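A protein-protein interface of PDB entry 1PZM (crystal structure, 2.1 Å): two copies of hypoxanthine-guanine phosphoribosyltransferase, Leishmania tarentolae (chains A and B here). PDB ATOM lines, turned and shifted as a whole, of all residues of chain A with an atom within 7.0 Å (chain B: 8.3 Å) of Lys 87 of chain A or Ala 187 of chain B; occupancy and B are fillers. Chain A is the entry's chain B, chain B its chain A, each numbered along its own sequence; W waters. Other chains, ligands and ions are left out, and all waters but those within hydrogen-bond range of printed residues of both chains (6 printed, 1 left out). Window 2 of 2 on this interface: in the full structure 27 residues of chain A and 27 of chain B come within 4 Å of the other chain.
The backbone carbonyl oxygen (O) of Val 88 of chain A sits at hydrogen-bond distance from the side-chain amino group (NZ) of Lys 66 of chain B, 2.5 Å away.
The side-chain carboxylate (OE1) of Glu 89 of chain A is in salt-bridge range of the side-chain amino group (NZ) of Lys 66 of chain B (3.3 Å).
OE2 of Glu 192 of chain B lies within hydrogen-bond range of N of Val 86 of chain A (3.1 Å).
N of Glu 188 of chain B lies within hydrogen-bond range of OD2 of Asp 185 of chain B (2.8 Å).
OE1 of Glu 192 of chain B lies close to N of Tyr 190 of chain B (3.3 Å).
O of Pro 85 of chain A sits at hydrogen-bond distance from N of Leu 59 of chain A.
N of Lys 87 of chain A is in hydrogen-bond range of O of Leu 59 of chain A (3.0 Å).
The backbone carbonyl oxygen (O) of Lys 87 of chain A sits at hydrogen-bond distance from the backbone NH (N) of Leu 61 of chain A (2.9 Å).
O of Leu 61 of chain A sits at hydrogen-bond distance from N of Glu 89 of chain A.
Among the printed residues, pairs that only touch across the chains: Ala 55 of chain A with Ser 189 of chain B (3.5 Å), Val 84 of chain A with Glu 192 of chain B (3.9 Å), Pro 85 of chain A with Glu 192 of chain B (3.6 Å), Lys 87 of chain A with Ala 187 of chain B (3.7 Å), Lys 87 of chain A with Glu 188 of chain B (3.4 Å) and Lys 87 of chain A with Ser 189 of chain B (3.3 Å).
Printed residues of chain B within 4 Å of Ala 55 of chain A: Ser 189.
Of the printed residues of chain B, Pro 85 of chain A touches Glu 192.
Lys 87 of chain A touches just these residues of chain B: Ala 187, Glu 188 and Ser 189.
Of the printed residues of chain B, Val 88 of chain A touches Lys 66.
Of the printed residues of chain A, Lys 66 of chain B touches Val 88 (2.5 Å) and Glu 89 (3.3 Å).
Ala 187 of chain B touches one residue of chain A.
Printed residues of chain A within 4 Å of Glu 188 of chain B: Lys 87.
The nearest residue of chain B that does not touch Lys 87 of chain A is Glu 192 of chain B (5.5 Å).
The nearest printed residue of chain B that does not touch Val 84 of chain A is Tyr 190 of chain B (8.3 Å).
Of the 16 printed residues of chain A, 7 touch a printed residue of chain B.
Hydrophobic or aromatic side chains of chain A that line the printed part of chain B: Ala 55 and Val 86.
Of the 14 printed residues of chain B, 5 touch a printed residue of chain A.
Printed residues of chain B that touch a printed residue of chain A: Lys 66, Ala 187, Glu 188, Ser 189 and Glu 192.
No position is printed for both chains.
Water W1 lies within hydrogen-bond range of OG of Ser 189 of chain B (2.6 Å), O of Ala 187 of chain B (2.8 Å) and NZ of Lys 87 of chain A (3.4 Å).
Water W3 lies within hydrogen-bond range of the backbone carbonyl oxygen of Glu 188 of chain B (2.6 Å), the backbone NH of Val 88 of chain A (2.8 Å) and the guanidinium group of Arg 191 of chain B (3.0 Å).
Water W6 bridges the side-chain carboxylate of Glu 89 of chain A and the side-chain amino group of Lys 66 of chain B.
Water W5 bridges the side-chain carboxylate of Glu 192 of chain B (2.7 Å) and the backbone carbonyl oxygen of Val 84 of chain A (2.9 Å).
Water W2 lies within hydrogen-bond range of OG of Ser 189 of chain B, O of Val 86 of chain A and O of Ala 55 of chain A.
Water W4 lies within hydrogen-bond range of the side-chain amino group of Lys 66 of chain B (2.9 Å), the side-chain carboxylate of Glu 89 of chain A (3.0 Å) and the side-chain carboxylate of Glu 188 of chain B (3.0 Å).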
ATOM      1  N   THR A  54       2.221  15.159  -8.837  1.00  0.00           N
ATOM      2  CA  THR A  54       2.981  16.265  -8.247  1.00  0.00           C
ATOM      3  C   THR A  54       2.583  17.468  -9.056  1.00  0.00           C
ATOM      4  O   THR A  54       1.880  17.327 -10.066  1.00  0.00           O
ATOM      5  CB  THR A  54       4.469  16.074  -8.463  1.00  0.00           C
ATOM      6  OG1 THR A  54       4.694  16.083  -9.882  1.00  0.00           O
ATOM      7  CG2 THR A  54       4.946  14.685  -8.002  1.00  0.00           C
ATOM      8  N   ALA A  55       3.117  18.629  -8.690  1.00  0.00           N
ATOM      9  CA  ALA A  55       2.889  19.865  -9.466  1.00  0.00           C
ATOM     10  C   ALA A  55       3.308  19.731 -10.917  1.00  0.00           C
ATOM     11  O   ALA A  55       2.617  20.204 -11.816  1.00  0.00           O
ATOM     12  CB  ALA A  55       3.582  21.118  -8.778  1.00  0.00           C
ATOM     13  N   ASP A  56       4.419  19.045 -11.140  1.00  0.00           N
ATOM     14  CA  ASP A  56       4.961  18.817 -12.476  1.00  0.00           C
ATOM     15  C   ASP A  56       4.254  17.706 -13.292  1.00  0.00           C
ATOM     16  O   ASP A  56       4.344  17.680 -14.541  1.00  0.00           O
ATOM     17  CB  ASP A  56       6.441  18.490 -12.384  1.00  0.00           C
ATOM     18  CG  ASP A  56       7.147  18.692 -13.691  1.00  0.00           C
ATOM     19  OD1 ASP A  56       6.903  19.753 -14.338  1.00  0.00           O
ATOM     20  OD2 ASP A  56       7.962  17.853 -14.130  1.00  0.00           O
ATOM     21  N   ASN A  57       3.547  16.842 -12.576  1.00  0.00           N
ATOM     22  CA  ASN A  57       2.790  15.749 -13.144  1.00  0.00           C
ATOM     23  C   ASN A  57       1.467  15.646 -12.416  1.00  0.00           C
ATOM     24  O   ASN A  57       1.260  14.789 -11.559  1.00  0.00           O
ATOM     25  CB  ASN A  57       3.576  14.428 -13.085  1.00  0.00           C
ATOM     26  CG  ASN A  57       2.782  13.264 -13.645  1.00  0.00           C
ATOM     27  OD1 ASN A  57       1.979  13.418 -14.611  1.00  0.00           O
ATOM     28  ND2 ASN A  57       2.923  12.124 -12.995  1.00  0.00           N
ATOM     29  N   PRO A  58       0.596  16.604 -12.699  1.00  0.00           N
ATOM     30  CA  PRO A  58      -0.623  16.779 -11.928  1.00  0.00           C
ATOM     31  C   PRO A  58      -1.838  16.179 -12.571  1.00  0.00           C
ATOM     32  O   PRO A  58      -1.747  15.662 -13.687  1.00  0.00           O
ATOM     33  CB  PRO A  58      -0.799  18.326 -11.945  1.00  0.00           C
ATOM     34  CG  PRO A  58      -0.326  18.727 -13.345  1.00  0.00           C
ATOM     35  CD  PRO A  58       0.769  17.677 -13.740  1.00  0.00           C
ATOM     36  N   LEU A  59      -2.976  16.309 -11.892  1.00  0.00           N
ATOM     37  CA  LEU A  59      -4.238  16.049 -12.562  1.00  0.00           C
ATOM     38  C   LEU A  59      -4.654  17.271 -13.361  1.00  0.00           C
ATOM     39  O   LEU A  59      -4.880  18.360 -12.785  1.00  0.00           O
ATOM     40  CB  LEU A  59      -5.339  15.688 -11.550  1.00  0.00           C
ATOM     41  CG  LEU A  59      -6.716  15.337 -12.140  1.00  0.00           C
ATOM     42  CD1 LEU A  59      -6.652  14.185 -13.108  1.00  0.00           C
ATOM     43  CD2 LEU A  59      -7.778  15.023 -10.989  1.00  0.00           C
ATOM     44  N   TYR A  60      -4.782  17.081 -14.681  1.00  0.00           N
ATOM     45  CA  TYR A  60      -5.306  18.126 -15.574  1.00  0.00           C
ATOM     46  C   TYR A  60      -6.856  18.077 -15.630  1.00  0.00           C
ATOM     47  O   TYR A  60      -7.445  17.084 -16.094  1.00  0.00           O
ATOM     48  CB  TYR A  60      -4.741  17.996 -17.022  1.00  0.00           C
ATOM     49  CG  TYR A  60      -3.306  18.456 -17.199  1.00  0.00           C
ATOM     50  CD1 TYR A  60      -2.234  17.623 -16.836  1.00  0.00           C
ATOM     51  CD2 TYR A  60      -3.001  19.713 -17.764  1.00  0.00           C
ATOM     52  CE1 TYR A  60      -0.909  18.032 -17.000  1.00  0.00           C
ATOM     53  CE2 TYR A  60      -1.658  20.132 -17.930  1.00  0.00           C
ATOM     54  CZ  TYR A  60      -0.635  19.263 -17.545  1.00  0.00           C
ATOM     55  OH  TYR A  60       0.684  19.628 -17.664  1.00  0.00           O
ATOM     56  N   LEU A  61      -7.496  19.157 -15.222  1.00  0.00           N
ATOM     57  CA  LEU A  61      -8.936  19.297 -15.354  1.00  0.00           C
ATOM     58  C   LEU A  61      -9.235  20.046 -16.645  1.00  0.00           C
ATOM     59  O   LEU A  61      -8.866  21.223 -16.787  1.00  0.00           O
ATOM     60  CB  LEU A  61      -9.486  20.138 -14.174  1.00  0.00           C
ATOM     61  CG  LEU A  61      -9.280  19.517 -12.790  1.00  0.00           C
ATOM     62  CD1 LEU A  61      -9.840  20.509 -11.693  1.00  0.00           C
ATOM     63  CD2 LEU A  61     -10.004  18.133 -12.576  1.00  0.00           C
ATOM     64  N   LEU A  62      -9.944  19.383 -17.547  1.00  0.00           N
ATOM     65  CA  LEU A  62     -10.352  19.964 -18.821  1.00  0.00           C
ATOM     66  C   LEU A  62     -11.823  20.420 -18.646  1.00  0.00           C
ATOM     67  O   LEU A  62     -12.786  19.652 -18.795  1.00  0.00           O
ATOM     68  CB  LEU A  62     -10.248  18.907 -19.983  1.00  0.00           C
ATOM     69  CG  LEU A  62      -8.850  18.878 -20.643  1.00  0.00           C
ATOM     70  CD1 LEU A  62      -7.659  18.768 -19.668  1.00  0.00           C
ATOM     71  CD2 LEU A  62      -8.771  17.732 -21.690  1.00  0.00           C
ATOM     72  N   VAL A  84      -4.652  16.972  -3.942  1.00  0.00           N
ATOM     73  CA  VAL A  84      -4.451  16.549  -5.334  1.00  0.00           C
ATOM     74  C   VAL A  84      -3.959  17.796  -6.125  1.00  0.00           C
ATOM     75  O   VAL A  84      -4.705  18.751  -6.274  1.00  0.00           O
ATOM     76  CB  VAL A  84      -5.741  16.001  -5.973  1.00  0.00           C
ATOM     77  CG1 VAL A  84      -5.471  15.640  -7.442  1.00  0.00           C
ATOM     78  CG2 VAL A  84      -6.240  14.769  -5.216  1.00  0.00           C
ATOM     79  N   PRO A  85      -2.727  17.782  -6.626  1.00  0.00           N
ATOM     80  CA  PRO A  85      -2.227  18.919  -7.421  1.00  0.00           C
ATOM     81  C   PRO A  85      -2.949  18.960  -8.794  1.00  0.00           C
ATOM     82  O   PRO A  85      -3.174  17.887  -9.433  1.00  0.00           O
ATOM     83  CB  PRO A  85      -0.726  18.619  -7.579  1.00  0.00           C
ATOM     84  CG  PRO A  85      -0.598  17.082  -7.388  1.00  0.00           C
ATOM     85  CD  PRO A  85      -1.765  16.645  -6.570  1.00  0.00           C
ATOM     86  N   VAL A  86      -3.390  20.147  -9.215  1.00  0.00           N
ATOM     87  CA  VAL A  86      -4.080  20.219 -10.514  1.00  0.00           C
ATOM     88  C   VAL A  86      -3.561  21.286 -11.438  1.00  0.00           C
ATOM     89  O   VAL A  86      -2.884  22.237 -11.007  1.00  0.00           O
ATOM     90  CB  VAL A  86      -5.655  20.365 -10.406  1.00  0.00           C
ATOM     91  CG1 VAL A  86      -6.277  19.497  -9.271  1.00  0.00           C
ATOM     92  CG2 VAL A  86      -6.083  21.739 -10.275  1.00  0.00           C
ATOM     93  N   LYS A  87      -3.862  21.130 -12.719  1.00  0.00           N
ATOM     94  CA  LYS A  87      -3.682  22.217 -13.655  1.00  0.00           C
ATOM     95  C   LYS A  87      -5.006  22.282 -14.382  1.00  0.00           C
ATOM     96  O   LYS A  87      -5.748  21.299 -14.375  1.00  0.00           O
ATOM     97  CB  LYS A  87      -2.503  21.945 -14.627  1.00  0.00           C
ATOM     98  CG  LYS A  87      -1.101  22.170 -13.969  1.00  0.00           C
ATOM     99  CD  LYS A  87       0.119  22.084 -14.919  1.00  0.00           C
ATOM    100  CE  LYS A  87       1.436  22.302 -14.121  1.00  0.00           C
ATOM    101  NZ  LYS A  87       2.672  22.149 -15.002  1.00  0.00           N
ATOM    102  N   VAL A  88      -5.313  23.439 -14.968  1.00  0.00           N
ATOM    103  CA  VAL A  88      -6.608  23.653 -15.603  1.00  0.00           C
ATOM    104  C   VAL A  88      -6.509  24.092 -17.061  1.00  0.00           C
ATOM    105  O   VAL A  88      -5.675  24.952 -17.417  1.00  0.00           O
ATOM    106  CB  VAL A  88      -7.440  24.726 -14.824  1.00  0.00           C
ATOM    107  CG1 VAL A  88      -8.873  24.746 -15.347  1.00  0.00           C
ATOM    108  CG2 VAL A  88      -7.462  24.404 -13.246  1.00  0.00           C
ATOM    109  N   GLU A  89      -7.375  23.530 -17.896  1.00  0.00           N
ATOM    110  CA  GLU A  89      -7.455  23.868 -19.336  1.00  0.00           C
ATOM    111  C   GLU A  89      -8.943  24.071 -19.649  1.00  0.00           C
ATOM    112  O   GLU A  89      -9.844  23.541 -18.949  1.00  0.00           O
ATOM    113  CB  GLU A  89      -7.008  22.640 -20.220  1.00  0.00           C
ATOM    114  CG  GLU A  89      -5.566  22.149 -20.034  1.00  0.00           C
ATOM    115  CD  GLU A  89      -4.508  23.168 -20.444  1.00  0.00           C
ATOM    116  OE1 GLU A  89      -4.831  24.163 -21.150  1.00  0.00           O
ATOM    117  OE2 GLU A  89      -3.344  23.019 -20.008  1.00  0.00           O
ATOM    118  N   ARG A 119      -0.002  12.961 -20.214  1.00  0.00           N
ATOM    119  CA  ARG A 119      -0.531  13.641 -19.016  1.00  0.00           C
ATOM    120  C   ARG A 119      -1.755  12.892 -18.517  1.00  0.00           C
ATOM    121  O   ARG A 119      -2.444  12.180 -19.325  1.00  0.00           O
ATOM    122  CB  ARG A 119      -0.982  15.083 -19.324  1.00  0.00           C
ATOM    123  CG  ARG A 119       0.137  15.924 -19.880  1.00  0.00           C
ATOM    124  CD  ARG A 119       1.384  15.831 -19.059  1.00  0.00           C
ATOM    125  NE  ARG A 119       2.330  16.911 -19.361  1.00  0.00           N
ATOM    126  CZ  ARG A 119       3.364  17.219 -18.582  1.00  0.00           C
ATOM    127  NH1 ARG A 119       3.576  16.511 -17.451  1.00  0.00           N
ATOM    128  NH2 ARG A 119       4.185  18.205 -18.947  1.00  0.00           N
ATOM    129  N   LYS B  66      -6.959  32.490 -18.182  1.00  0.00           N
ATOM    130  CA  LYS B  66      -7.472  31.375 -17.339  1.00  0.00           C
ATOM    131  C   LYS B  66      -7.827  31.845 -15.971  1.00  0.00           C
ATOM    132  O   LYS B  66      -8.739  31.349 -15.353  1.00  0.00           O
ATOM    133  CB  LYS B  66      -6.361  30.328 -17.178  1.00  0.00           C
ATOM    134  CG  LYS B  66      -5.997  29.491 -18.473  1.00  0.00           C
ATOM    135  CD  LYS B  66      -5.084  28.289 -18.087  1.00  0.00           C
ATOM    136  CE  LYS B  66      -4.688  27.393 -19.254  1.00  0.00           C
ATOM    137  NZ  LYS B  66      -3.950  26.224 -18.687  1.00  0.00           N
ATOM    138  N   PHE B  69     -11.234  32.553 -13.811  1.00  0.00           N
ATOM    139  CA  PHE B  69     -12.372  31.622 -13.700  1.00  0.00           C
ATOM    140  C   PHE B  69     -12.952  31.386 -12.310  1.00  0.00           C
ATOM    141  O   PHE B  69     -14.197  31.222 -12.176  1.00  0.00           O
ATOM    142  CB  PHE B  69     -12.164  30.281 -14.451  1.00  0.00           C
ATOM    143  CG  PHE B  69     -11.513  29.177 -13.639  1.00  0.00           C
ATOM    144  CD1 PHE B  69     -12.246  28.028 -13.312  1.00  0.00           C
ATOM    145  CD2 PHE B  69     -10.137  29.233 -13.307  1.00  0.00           C
ATOM    146  CE1 PHE B  69     -11.642  26.950 -12.616  1.00  0.00           C
ATOM    147  CE2 PHE B  69      -9.523  28.195 -12.604  1.00  0.00           C
ATOM    148  CZ  PHE B  69     -10.286  27.060 -12.228  1.00  0.00           C
ATOM    149  N   PHE B 178       4.258  38.724  -6.211  1.00  0.00           N
ATOM    150  CA  PHE B 178       3.676  37.760  -7.119  1.00  0.00           C
ATOM    151  C   PHE B 178       2.720  36.843  -6.346  1.00  0.00           C
ATOM    152  O   PHE B 178       3.131  36.170  -5.413  1.00  0.00           O
ATOM    153  CB  PHE B 178       4.754  36.997  -7.838  1.00  0.00           C
ATOM    154  CG  PHE B 178       4.221  36.134  -8.937  1.00  0.00           C
ATOM    155  CD1 PHE B 178       3.740  34.860  -8.663  1.00  0.00           C
ATOM    156  CD2 PHE B 178       4.171  36.604 -10.228  1.00  0.00           C
ATOM    157  CE1 PHE B 178       3.262  34.050  -9.689  1.00  0.00           C
ATOM    158  CE2 PHE B 178       3.696  35.815 -11.247  1.00  0.00           C
ATOM    159  CZ  PHE B 178       3.230  34.529 -10.972  1.00  0.00           C
ATOM    160  N   ILE B 180      -0.351  33.687  -6.007  1.00  0.00           N
ATOM    161  CA  ILE B 180      -0.858  32.432  -6.553  1.00  0.00           C
ATOM    162  C   ILE B 180      -2.143  32.117  -5.761  1.00  0.00           C
ATOM    163  O   ILE B 180      -2.405  32.758  -4.725  1.00  0.00           O
ATOM    164  CB  ILE B 180       0.192  31.287  -6.375  1.00  0.00           C
ATOM    165  CG1 ILE B 180       0.444  31.075  -4.855  1.00  0.00           C
ATOM    166  CG2 ILE B 180       1.526  31.618  -7.166  1.00  0.00           C
ATOM    167  CD1 ILE B 180       1.194  29.827  -4.478  1.00  0.00           C
ATOM    168  N   MET B 184      -5.151  31.871  -9.690  1.00  0.00           N
ATOM    169  CA  MET B 184      -3.908  32.469 -10.259  1.00  0.00           C
ATOM    170  C   MET B 184      -2.776  31.469 -10.091  1.00  0.00           C
ATOM    171  O   MET B 184      -2.699  30.787  -9.049  1.00  0.00           O
ATOM    172  CB  MET B 184      -3.557  33.777  -9.504  1.00  0.00           C
ATOM    173  CG  MET B 184      -4.637  34.862  -9.799  1.00  0.00           C
ATOM    174  SD  MET B 184      -4.752  36.310  -8.693  1.00  0.00           S
ATOM    175  CE  MET B 184      -5.722  35.472  -7.319  1.00  0.00           C
ATOM    176  N   ASP B 185      -1.877  31.400 -11.052  1.00  0.00           N
ATOM    177  CA  ASP B 185      -0.958  30.268 -11.122  1.00  0.00           C
ATOM    178  C   ASP B 185       0.495  30.691 -10.947  1.00  0.00           C
ATOM    179  O   ASP B 185       0.828  31.903 -11.060  1.00  0.00           O
ATOM    180  CB  ASP B 185      -1.056  29.610 -12.481  1.00  0.00           C
ATOM    181  CG  ASP B 185      -0.439  30.474 -13.596  1.00  0.00           C
ATOM    182  OD1 ASP B 185      -0.793  31.655 -13.698  1.00  0.00           O
ATOM    183  OD2 ASP B 185       0.397  30.028 -14.396  1.00  0.00           O
ATOM    184  N   PHE B 186       1.354  29.712 -10.681  1.00  0.00           N
ATOM    185  CA  PHE B 186       2.773  29.885 -10.996  1.00  0.00           C
ATOM    186  C   PHE B 186       3.105  28.739 -11.938  1.00  0.00           C
ATOM    187  O   PHE B 186       2.952  27.566 -11.567  1.00  0.00           O
ATOM    188  CB  PHE B 186       3.707  29.869  -9.788  1.00  0.00           C
ATOM    189  CG  PHE B 186       5.186  29.886 -10.193  1.00  0.00           C
ATOM    190  CD1 PHE B 186       5.756  31.025 -10.708  1.00  0.00           C
ATOM    191  CD2 PHE B 186       5.973  28.732 -10.088  1.00  0.00           C
ATOM    192  CE1 PHE B 186       7.098  31.033 -11.082  1.00  0.00           C
ATOM    193  CE2 PHE B 186       7.297  28.733 -10.429  1.00  0.00           C
ATOM    194  CZ  PHE B 186       7.871  29.860 -10.944  1.00  0.00           C
ATOM    195  N   ALA B 187       3.555  29.060 -13.150  1.00  0.00           N
ATOM    196  CA  ALA B 187       3.816  28.005 -14.187  1.00  0.00           C
ATOM    197  C   ALA B 187       2.640  26.956 -14.328  1.00  0.00           C
ATOM    198  O   ALA B 187       2.871  25.768 -14.349  1.00  0.00           O
ATOM    199  CB  ALA B 187       5.144  27.292 -13.897  1.00  0.00           C
ATOM    200  N   GLU B 188       1.391  27.449 -14.295  1.00  0.00           N
ATOM    201  CA  GLU B 188       0.155  26.673 -14.479  1.00  0.00           C
ATOM    202  C   GLU B 188      -0.324  25.975 -13.198  1.00  0.00           C
ATOM    203  O   GLU B 188      -1.462  25.444 -13.186  1.00  0.00           O
ATOM    204  CB  GLU B 188       0.231  25.665 -15.671  1.00  0.00           C
ATOM    205  CG  GLU B 188       0.446  26.345 -17.041  1.00  0.00           C
ATOM    206  CD  GLU B 188      -0.672  27.345 -17.392  1.00  0.00           C
ATOM    207  OE1 GLU B 188      -1.814  27.230 -16.904  1.00  0.00           O
ATOM    208  OE2 GLU B 188      -0.424  28.294 -18.145  1.00  0.00           O
ATOM    209  N   SER B 189       0.536  25.938 -12.171  1.00  0.00           N
ATOM    210  CA  SER B 189       0.199  25.262 -10.890  1.00  0.00           C
ATOM    211  C   SER B 189      -0.434  26.245  -9.905  1.00  0.00           C
ATOM    212  O   SER B 189      -0.324  27.465 -10.100  1.00  0.00           O
ATOM    213  CB  SER B 189       1.432  24.592 -10.248  1.00  0.00           C
ATOM    214  OG  SER B 189       1.928  23.560 -11.069  1.00  0.00           O
ATOM    215  N   TYR B 190      -1.112  25.712  -8.875  1.00  0.00           N
ATOM    216  CA  TYR B 190      -1.580  26.483  -7.717  1.00  0.00           C
ATOM    217  C   TYR B 190      -2.855  27.260  -7.924  1.00  0.00           C
ATOM    218  O   TYR B 190      -3.323  27.891  -6.993  1.00  0.00           O
ATOM    219  CB  TYR B 190      -0.476  27.411  -7.153  1.00  0.00           C
ATOM    220  CG  TYR B 190       0.842  26.690  -7.018  1.00  0.00           C
ATOM    221  CD1 TYR B 190       0.894  25.404  -6.478  1.00  0.00           C
ATOM    222  CD2 TYR B 190       2.038  27.277  -7.444  1.00  0.00           C
ATOM    223  CE1 TYR B 190       2.118  24.717  -6.375  1.00  0.00           C
ATOM    224  CE2 TYR B 190       3.277  26.591  -7.324  1.00  0.00           C
ATOM    225  CZ  TYR B 190       3.294  25.323  -6.778  1.00  0.00           C
ATOM    226  OH  TYR B 190       4.450  24.596  -6.652  1.00  0.00           O
ATOM    227  N   ARG B 191      -3.458  27.190  -9.101  1.00  0.00           N
ATOM    228  CA  ARG B 191      -4.764  27.849  -9.310  1.00  0.00           C
ATOM    229  C   ARG B 191      -5.849  27.345  -8.377  1.00  0.00           C
ATOM    230  O   ARG B 191      -6.792  28.065  -8.109  1.00  0.00           O
ATOM    231  CB  ARG B 191      -5.318  27.535 -10.718  1.00  0.00           C
ATOM    232  CG  ARG B 191      -4.450  28.136 -11.869  1.00  0.00           C
ATOM    233  CD  ARG B 191      -5.185  28.053 -13.198  1.00  0.00           C
ATOM    234  NE  ARG B 191      -4.275  28.340 -14.290  1.00  0.00           N
ATOM    235  CZ  ARG B 191      -3.898  29.563 -14.685  1.00  0.00           C
ATOM    236  NH1 ARG B 191      -4.359  30.669 -14.083  1.00  0.00           N
ATOM    237  NH2 ARG B 191      -3.062  29.692 -15.701  1.00  0.00           N
ATOM    238  N   GLU B 192      -5.736  26.070  -7.992  1.00  0.00           N
ATOM    239  CA  GLU B 192      -6.768  25.433  -7.123  1.00  0.00           C
ATOM    240  C   GLU B 192      -6.769  25.827  -5.632  1.00  0.00           C
ATOM    241  O   GLU B 192      -7.728  25.501  -4.840  1.00  0.00           O
ATOM    242  CB  GLU B 192      -6.678  23.895  -7.312  1.00  0.00           C
ATOM    243  CG  GLU B 192      -5.526  23.201  -6.614  1.00  0.00           C
ATOM    244  CD  GLU B 192      -4.177  23.230  -7.333  1.00  0.00           C
ATOM    245  OE1 GLU B 192      -3.948  24.164  -8.136  1.00  0.00           O
ATOM    246  OE2 GLU B 192      -3.315  22.351  -7.054  1.00  0.00           O
ATOM    247  N   LEU B 199       3.948  33.890  -3.309  1.00  0.00           N
ATOM    248  CA  LEU B 199       4.767  32.714  -3.675  1.00  0.00           C
ATOM    249  C   LEU B 199       6.156  32.767  -2.992  1.00  0.00           C
ATOM    250  O   LEU B 199       6.848  33.814  -3.044  1.00  0.00           O
ATOM    251  CB  LEU B 199       4.905  32.629  -5.212  1.00  0.00           C
ATOM    252  CG  LEU B 199       5.747  31.472  -5.763  1.00  0.00           C
ATOM    253  CD1 LEU B 199       5.065  30.090  -5.611  1.00  0.00           C
ATOM    254  CD2 LEU B 199       6.119  31.715  -7.207  1.00  0.00           C
HETATM  255  O   HOH W   1       4.008  24.057 -12.466  1.00  0.00           O
HETATM  256  O   HOH W   2      -0.036  21.642 -10.341  1.00  0.00           O
HETATM  257  O   HOH W   3      -3.369  25.513 -14.969  1.00  0.00           O
HETATM  258  O   HOH W   4      -2.180  24.297 -17.556  1.00  0.00           O
HETATM  259  O   HOH W   5      -3.585  20.965  -4.807  1.00  0.00           O
HETATM  260  O   HOH W   6      -2.544  25.402 -21.623  1.00  0.00           O
